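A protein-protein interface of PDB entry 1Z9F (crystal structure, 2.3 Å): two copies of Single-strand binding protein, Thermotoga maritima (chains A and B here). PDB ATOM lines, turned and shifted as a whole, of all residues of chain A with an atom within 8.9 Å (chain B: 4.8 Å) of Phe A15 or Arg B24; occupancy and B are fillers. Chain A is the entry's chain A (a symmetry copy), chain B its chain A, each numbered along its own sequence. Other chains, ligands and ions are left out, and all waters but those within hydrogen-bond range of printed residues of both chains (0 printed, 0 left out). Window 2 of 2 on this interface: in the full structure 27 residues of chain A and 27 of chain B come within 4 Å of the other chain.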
ATOM      1  N   HIS A  12     -35.468 -11.981 -25.652  1.00  0.00           N
ATOM      2  CA  HIS A  12     -34.793 -13.280 -25.311  1.00  0.00           C
ATOM      3  C   HIS A  12     -33.639 -13.564 -26.272  1.00  0.00           C
ATOM      4  O   HIS A  12     -33.603 -13.006 -27.385  1.00  0.00           O
ATOM      5  CB  HIS A  12     -35.785 -14.457 -25.369  1.00  0.00           C
ATOM      6  CG  HIS A  12     -35.966 -15.035 -26.747  1.00  0.00           C
ATOM      7  ND1 HIS A  12     -37.002 -14.671 -27.586  1.00  0.00           N
ATOM      8  CD2 HIS A  12     -35.227 -15.943 -27.436  1.00  0.00           C
ATOM      9  CE1 HIS A  12     -36.890 -15.327 -28.730  1.00  0.00           C
ATOM     10  NE2 HIS A  12     -35.822 -16.104 -28.666  1.00  0.00           N
ATOM     11  N   MET A  13     -32.739 -14.459 -25.851  1.00  0.00           N
ATOM     12  CA  MET A  13     -31.637 -14.971 -26.687  1.00  0.00           C
ATOM     13  C   MET A  13     -30.662 -15.841 -25.866  1.00  0.00           C
ATOM     14  O   MET A  13     -30.448 -17.007 -26.210  1.00  0.00           O
ATOM     15  CB  MET A  13     -30.863 -13.825 -27.357  1.00  0.00           C
ATOM     16  CG  MET A  13     -29.922 -14.237 -28.479  1.00  0.00           C
ATOM     17  SD  MET A  13     -29.223 -12.776 -29.309  1.00  0.00           S
ATOM     18  CE  MET A  13     -30.319 -12.691 -30.744  1.00  0.00           C
ATOM     19  N   SER A  14     -30.089 -15.252 -24.804  1.00  0.00           N
ATOM     20  CA  SER A  14     -29.139 -15.899 -23.848  1.00  0.00           C
ATOM     21  C   SER A  14     -27.679 -15.461 -24.066  1.00  0.00           C
ATOM     22  O   SER A  14     -26.739 -16.125 -23.628  1.00  0.00           O
ATOM     23  CB  SER A  14     -29.238 -17.428 -23.861  1.00  0.00           C
ATOM     24  OG  SER A  14     -28.582 -17.987 -22.742  1.00  0.00           O
ATOM     25  N   PHE A  15     -27.512 -14.327 -24.734  1.00  0.00           N
ATOM     26  CA  PHE A  15     -26.223 -13.802 -25.124  1.00  0.00           C
ATOM     27  C   PHE A  15     -26.284 -12.287 -24.980  1.00  0.00           C
ATOM     28  O   PHE A  15     -27.366 -11.738 -24.811  1.00  0.00           O
ATOM     29  CB  PHE A  15     -25.914 -14.198 -26.565  1.00  0.00           C
ATOM     30  CG  PHE A  15     -25.749 -15.683 -26.756  1.00  0.00           C
ATOM     31  CD1 PHE A  15     -24.514 -16.291 -26.539  1.00  0.00           C
ATOM     32  CD2 PHE A  15     -26.830 -16.482 -27.133  1.00  0.00           C
ATOM     33  CE1 PHE A  15     -24.351 -17.673 -26.701  1.00  0.00           C
ATOM     34  CE2 PHE A  15     -26.678 -17.873 -27.302  1.00  0.00           C
ATOM     35  CZ  PHE A  15     -25.432 -18.465 -27.084  1.00  0.00           C
ATOM     36  N   PHE A  16     -25.141 -11.610 -25.030  1.00  0.00           N
ATOM     37  CA  PHE A  16     -25.102 -10.186 -24.775  1.00  0.00           C
ATOM     38  C   PHE A  16     -23.814  -9.612 -25.282  1.00  0.00           C
ATOM     39  O   PHE A  16     -22.786 -10.223 -25.188  1.00  0.00           O
ATOM     40  CB  PHE A  16     -25.251  -9.906 -23.277  1.00  0.00           C
ATOM     41  CG  PHE A  16     -25.399  -8.445 -22.935  1.00  0.00           C
ATOM     42  CD1 PHE A  16     -26.524  -7.748 -23.332  1.00  0.00           C
ATOM     43  CD2 PHE A  16     -24.427  -7.771 -22.221  1.00  0.00           C
ATOM     44  CE1 PHE A  16     -26.696  -6.421 -23.026  1.00  0.00           C
ATOM     45  CE2 PHE A  16     -24.582  -6.432 -21.908  1.00  0.00           C
ATOM     46  CZ  PHE A  16     -25.743  -5.752 -22.331  1.00  0.00           C
ATOM     47  N   ASN A  17     -23.869  -8.424 -25.843  1.00  0.00           N
ATOM     48  CA  ASN A  17     -22.682  -7.831 -26.433  1.00  0.00           C
ATOM     49  C   ASN A  17     -22.827  -6.334 -26.324  1.00  0.00           C
ATOM     50  O   ASN A  17     -23.635  -5.769 -26.991  1.00  0.00           O
ATOM     51  CB  ASN A  17     -22.568  -8.282 -27.887  1.00  0.00           C
ATOM     52  CG  ASN A  17     -21.433  -7.634 -28.627  1.00  0.00           C
ATOM     53  OD1 ASN A  17     -21.013  -6.523 -28.315  1.00  0.00           O
ATOM     54  ND2 ASN A  17     -20.944  -8.326 -29.664  1.00  0.00           N
ATOM     55  N   LYS A  18     -22.054  -5.706 -25.446  1.00  0.00           N
ATOM     56  CA  LYS A  18     -22.188  -4.300 -25.224  1.00  0.00           C
ATOM     57  C   LYS A  18     -20.842  -3.674 -25.088  1.00  0.00           C
ATOM     58  O   LYS A  18     -20.019  -4.122 -24.270  1.00  0.00           O
ATOM     59  CB  LYS A  18     -22.952  -4.125 -23.930  1.00  0.00           C
ATOM     60  CG  LYS A  18     -23.412  -2.751 -23.620  1.00  0.00           C
ATOM     61  CD  LYS A  18     -23.998  -2.189 -24.751  1.00  0.00           C
ATOM     62  CE  LYS A  18     -24.908  -1.075 -24.494  1.00  0.00           C
ATOM     63  NZ  LYS A  18     -25.560  -0.749 -25.831  1.00  0.00           N
ATOM     64  N   GLU A  92     -22.229  -2.297 -30.225  1.00  0.00           N
ATOM     65  CA  GLU A  92     -21.829  -3.686 -30.179  1.00  0.00           C
ATOM     66  C   GLU A  92     -20.487  -3.883 -30.778  1.00  0.00           C
ATOM     67  O   GLU A  92     -20.094  -3.184 -31.696  1.00  0.00           O
ATOM     68  CB  GLU A  92     -22.850  -4.552 -30.863  1.00  0.00           C
ATOM     69  CG  GLU A  92     -24.040  -4.791 -30.022  1.00  0.00           C
ATOM     70  CD  GLU A  92     -25.067  -5.629 -30.734  1.00  0.00           C
ATOM     71  OE1 GLU A  92     -24.801  -5.950 -31.917  1.00  0.00           O
ATOM     72  OE2 GLU A  92     -26.137  -5.942 -30.130  1.00  0.00           O
ATOM     73  N   ILE B  22     -21.808 -11.776 -22.942  1.00  0.00           N
ATOM     74  CA  ILE B  22     -22.287 -13.055 -22.419  1.00  0.00           C
ATOM     75  C   ILE B  22     -22.254 -14.068 -23.569  1.00  0.00           C
ATOM     76  O   ILE B  22     -22.944 -13.888 -24.576  1.00  0.00           O
ATOM     77  CB  ILE B  22     -23.700 -12.976 -21.849  1.00  0.00           C
ATOM     78  CG1 ILE B  22     -23.718 -12.109 -20.596  1.00  0.00           C
ATOM     79  CG2 ILE B  22     -24.197 -14.358 -21.492  1.00  0.00           C
ATOM     80  CD1 ILE B  22     -25.096 -11.868 -20.044  1.00  0.00           C
ATOM     81  N   GLY B  23     -21.430 -15.108 -23.419  1.00  0.00           N
ATOM     82  CA  GLY B  23     -21.293 -16.128 -24.437  1.00  0.00           C
ATOM     83  C   GLY B  23     -20.818 -17.452 -23.888  1.00  0.00           C
ATOM     84  O   GLY B  23     -20.466 -17.560 -22.717  1.00  0.00           O
ATOM     85  N   ARG B  24     -20.828 -18.472 -24.749  1.00  0.00           N
ATOM     86  CA  ARG B  24     -20.353 -19.809 -24.384  1.00  0.00           C
ATOM     87  C   ARG B  24     -18.839 -19.836 -24.585  1.00  0.00           C
ATOM     88  O   ARG B  24     -18.322 -19.109 -25.432  1.00  0.00           O
ATOM     89  CB  ARG B  24     -20.980 -20.930 -25.245  1.00  0.00           C
ATOM     90  CG  ARG B  24     -22.392 -20.731 -25.834  1.00  0.00           C
ATOM     91  CD  ARG B  24     -23.543 -20.600 -24.822  1.00  0.00           C
ATOM     92  NE  ARG B  24     -23.536 -21.605 -23.755  1.00  0.00           N
ATOM     93  CZ  ARG B  24     -24.626 -22.134 -23.190  1.00  0.00           C
ATOM     94  NH1 ARG B  24     -24.488 -23.033 -22.223  1.00  0.00           N
ATOM     95  NH2 ARG B  24     -25.852 -21.778 -23.567  1.00  0.00           N
ATOM     96  N   LEU B  25     -18.136 -20.665 -23.811  1.00  0.00           N
ATOM     97  CA  LEU B  25     -16.729 -20.977 -24.090  1.00  0.00           C
ATOM     98  C   LEU B  25     -16.744 -22.014 -25.196  1.00  0.00           C
ATOM     99  O   LEU B  25     -17.363 -23.063 -25.036  1.00  0.00           O
ATOM    100  CB  LEU B  25     -16.006 -21.568 -22.878  1.00  0.00           C
ATOM    101  CG  LEU B  25     -15.164 -20.634 -22.015  1.00  0.00           C
ATOM    102  CD1 LEU B  25     -16.048 -19.896 -21.021  1.00  0.00           C
ATOM    103  CD2 LEU B  25     -14.058 -21.419 -21.288  1.00  0.00           C
ATOM    104  N   VAL B  26     -16.078 -21.729 -26.313  1.00  0.00           N
ATOM    105  CA  VAL B  26     -16.086 -22.652 -27.461  1.00  0.00           C
ATOM    106  C   VAL B  26     -14.908 -23.604 -27.436  1.00  0.00           C
ATOM    107  O   VAL B  26     -14.891 -24.574 -28.179  1.00  0.00           O
ATOM    108  CB  VAL B  26     -16.134 -21.925 -28.823  1.00  0.00           C
ATOM    109  CG1 VAL B  26     -17.541 -21.433 -29.089  1.00  0.00           C
ATOM    110  CG2 VAL B  26     -15.123 -20.780 -28.885  1.00  0.00           C
ATOM    111  N   THR B  44     -11.756 -18.166 -25.637  1.00  0.00           N
ATOM    112  CA  THR B  44     -12.523 -17.431 -26.603  1.00  0.00           C
ATOM    113  C   THR B  44     -13.948 -17.869 -26.394  1.00  0.00           C
ATOM    114  O   THR B  44     -14.223 -19.056 -26.178  1.00  0.00           O
ATOM    115  CB  THR B  44     -12.071 -17.685 -28.073  1.00  0.00           C
ATOM    116  OG1 THR B  44     -12.816 -18.769 -28.645  1.00  0.00           O
ATOM    117  CG2 THR B  44     -10.544 -17.977 -28.159  1.00  0.00           C
ATOM    118  N   ILE B  45     -14.846 -16.885 -26.420  1.00  0.00           N
ATOM    119  CA  ILE B  45     -16.262 -17.137 -26.247  1.00  0.00           C
ATOM    120  C   ILE B  45     -17.003 -16.902 -27.561  1.00  0.00           C
ATOM    121  O   ILE B  45     -16.552 -16.129 -28.420  1.00  0.00           O
ATOM    122  CB  ILE B  45     -16.864 -16.297 -25.094  1.00  0.00           C
ATOM    123  CG1 ILE B  45     -16.557 -14.805 -25.272  1.00  0.00           C
ATOM    124  CG2 ILE B  45     -16.329 -16.816 -23.747  1.00  0.00           C
ATOM    125  CD1 ILE B  45     -17.266 -13.921 -24.279  1.00  0.00           C
ATOM    126  N   ALA B  46     -18.118 -17.605 -27.727  1.00  0.00           N
ATOM    127  CA  ALA B  46     -18.979 -17.412 -28.876  1.00  0.00           C
ATOM    128  C   ALA B  46     -20.116 -16.560 -28.386  1.00  0.00           C
ATOM    129  O   ALA B  46     -20.849 -16.983 -27.494  1.00  0.00           O
ATOM    130  CB  ALA B  46     -19.498 -18.737 -29.396  1.00  0.00           C
ATOM    131  N   VAL B  47     -20.242 -15.357 -28.948  1.00  0.00           N
ATOM    132  CA  VAL B  47     -21.316 -14.425 -28.601  1.00  0.00           C
ATOM    133  C   VAL B  47     -22.176 -14.216 -29.833  1.00  0.00           C
ATOM    134  O   VAL B  47     -21.928 -13.309 -30.640  1.00  0.00           O
ATOM    135  CB  VAL B  47     -20.750 -13.053 -28.139  1.00  0.00           C
ATOM    136  CG1 VAL B  47     -21.890 -12.042 -27.848  1.00  0.00           C
ATOM    137  CG2 VAL B  47     -19.815 -13.222 -26.918  1.00  0.00           C
ATOM    138  N   ASP B  48     -23.182 -15.061 -30.012  1.00  0.00           N
ATOM    139  CA  ASP B  48     -23.952 -14.941 -31.241  1.00  0.00           C
ATOM    140  C   ASP B  48     -24.989 -13.820 -31.159  1.00  0.00           C
ATOM    141  O   ASP B  48     -25.468 -13.464 -30.086  1.00  0.00           O
ATOM    142  CB  ASP B  48     -24.503 -16.299 -31.791  1.00  0.00           C
ATOM    143  CG  ASP B  48     -25.345 -17.081 -30.785  1.00  0.00           C
ATOM    144  OD1 ASP B  48     -25.783 -16.485 -29.770  1.00  0.00           O
ATOM    145  OD2 ASP B  48     -25.566 -18.298 -31.036  1.00  0.00           O
ATOM    146  N   GLY B  84     -18.278 -24.936 -23.760  1.00  0.00           N
ATOM    147  CA  GLY B  84     -19.745 -24.956 -23.731  1.00  0.00           C
ATOM    148  C   GLY B  84     -20.349 -24.042 -22.679  1.00  0.00           C
ATOM    149  O   GLY B  84     -21.359 -23.382 -22.927  1.00  0.00           O
ATOM    150  N   ARG B  85     -19.731 -24.026 -21.501  1.00  0.00           N
ATOM    151  CA  ARG B  85     -20.161 -23.219 -20.360  1.00  0.00           C
ATOM    152  C   ARG B  85     -20.424 -21.747 -20.747  1.00  0.00           C
ATOM    153  O   ARG B  85     -19.637 -21.153 -21.480  1.00  0.00           O
ATOM    154  CB  ARG B  85     -19.074 -23.317 -19.275  1.00  0.00           C
ATOM    155  CG  ARG B  85     -19.374 -22.613 -17.974  1.00  0.00           C
ATOM    156  CD  ARG B  85     -20.250 -23.432 -17.064  1.00  0.00           C
ATOM    157  NE  ARG B  85     -19.502 -24.478 -16.376  1.00  0.00           N
ATOM    158  CZ  ARG B  85     -19.928 -25.115 -15.287  1.00  0.00           C
ATOM    159  NH1 ARG B  85     -21.107 -24.821 -14.743  1.00  0.00           N
ATOM    160  NH2 ARG B  85     -19.168 -26.056 -14.730  1.00  0.00           N
ATOM    161  N   LEU B  86     -21.531 -21.185 -20.250  1.00  0.00           N
ATOM    162  CA  LEU B  86     -21.965 -19.810 -20.569  1.00  0.00           C
ATOM    163  C   LEU B  86     -21.479 -18.824 -19.520  1.00  0.00           C
ATOM    164  O   LEU B  86     -21.848 -18.926 -18.350  1.00  0.00           O
ATOM    165  CB  LEU B  86     -23.496 -19.735 -20.627  1.00  0.00           C
ATOM    166  CG  LEU B  86     -24.162 -18.378 -20.913  1.00  0.00           C
ATOM    167  CD1 LEU B  86     -23.935 -17.938 -22.340  1.00  0.00           C
ATOM    168  CD2 LEU B  86     -25.650 -18.443 -20.631  1.00  0.00           C
ATOM    169  N   ASP B 120     -24.845 -20.159 -16.415  1.00  0.00           N
ATOM    170  CA  ASP B 120     -25.619 -21.406 -16.305  1.00  0.00           C
ATOM    171  C   ASP B 120     -25.493 -22.078 -14.930  1.00  0.00           C
ATOM    172  O   ASP B 120     -24.393 -22.320 -14.432  1.00  0.00           O
ATOM    173  CB  ASP B 120     -25.240 -22.391 -17.425  1.00  0.00           C
ATOM    174  CG  ASP B 120     -23.738 -22.513 -17.625  1.00  0.00           C
ATOM    175  OD1 ASP B 120     -22.978 -22.090 -16.730  1.00  0.00           O
ATOM    176  OD2 ASP B 120     -23.317 -23.021 -18.688  1.00  0.00           O
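N of Ile B22 is in hydrogen-bond range of O of Phe A16 (2.9 Å).
O of Arg B24 is in hydrogen-bond range of N of Ala B46 (2.8 Å). The guanidinium group (NE) of Arg B24 sits at hydrogen-bond distance from the backbone carbonyl oxygen (O) of Gly B84, 2.9 Å away. The guanidinium group (NH1) of Arg B24 lies within salt-bridge range of the side-chain carboxylate (OD2) of Asp B120 (3.7 Å). The backbone NH of Leu B86 lies within hydrogen-bond range of the side-chain carboxylate of Asp B120, at 3.0 Å.
Among the printed residues, pairs that only touch across the chains: Met A13 with Asp B48 (3.9 Å), Ser A14 with Ile B22 (3.8 Å), Ser A14 with Leu B86 (3.6 Å), Phe A15 with Ile B22 (3.3 Å), Phe A15 with Gly B23 (3.8 Å), Phe A15 with Arg B24 (3.6 Å), Phe A15 with Ala B46 (3.7 Å), Phe A15 with Asp B48 (2.8 Å), Phe A16 with Val B47 (3.3 Å) and Asn A17 with Val B47 (3.8 Å).
Printed residues of chain B within 4 Å of Met A13: Asp B48. Of the printed residues of chain B, Phe A15 touches Ile B22 (3.3 Å), Gly B23 (3.8 Å), Arg B24 (3.6 Å), Ala B46 (3.7 Å) and Asp B48 (2.8 Å). Of the printed residues of chain B, Phe A16 touches Ile B22 and Val B47. Printed residues of chain B within 4 Å of Asn A17: Val B47 (3.8 Å). Of chain A, only Phe A15 comes within 4 Å of Gly B23. Thr B44 touches none of the printed residues of chain A. Ala B46 touches one residue of chain A. Printed residues of chain A within 4 Å of Asp B48: Met A13 and Phe A15. Of the printed residues of chain A, Leu B86 touches Ser A14. The nearest printed residue of chain A that does not touch Arg B24 is Ser A14 (4.7 Å). The nearest printed residue of chain A that does not touch Asp B48 is Phe A16 (5.4 Å).
Of the 8 printed residues of chain A, 5 touch a printed residue of chain B. Hydrophobic or aromatic side chains of chain A that line the printed part of chain B: Met A13, Phe A15 and Phe A16. Along chain A the printed residues that touch a printed residue of chain B span positions 13 to 17. Printed residues of chain B that touch a printed residue of chain A: Ile B22, Gly B23, Arg B24, Ala B46, Val B47, Asp B48 and Leu B86. Among the printed residues, 11 pairs touch across the chains. Among the printed residues, no Asp or Glu carboxylate lies within 4 Å of a Lys or Arg side-chain nitrogen of the other chain.
No position is printed for both chains.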
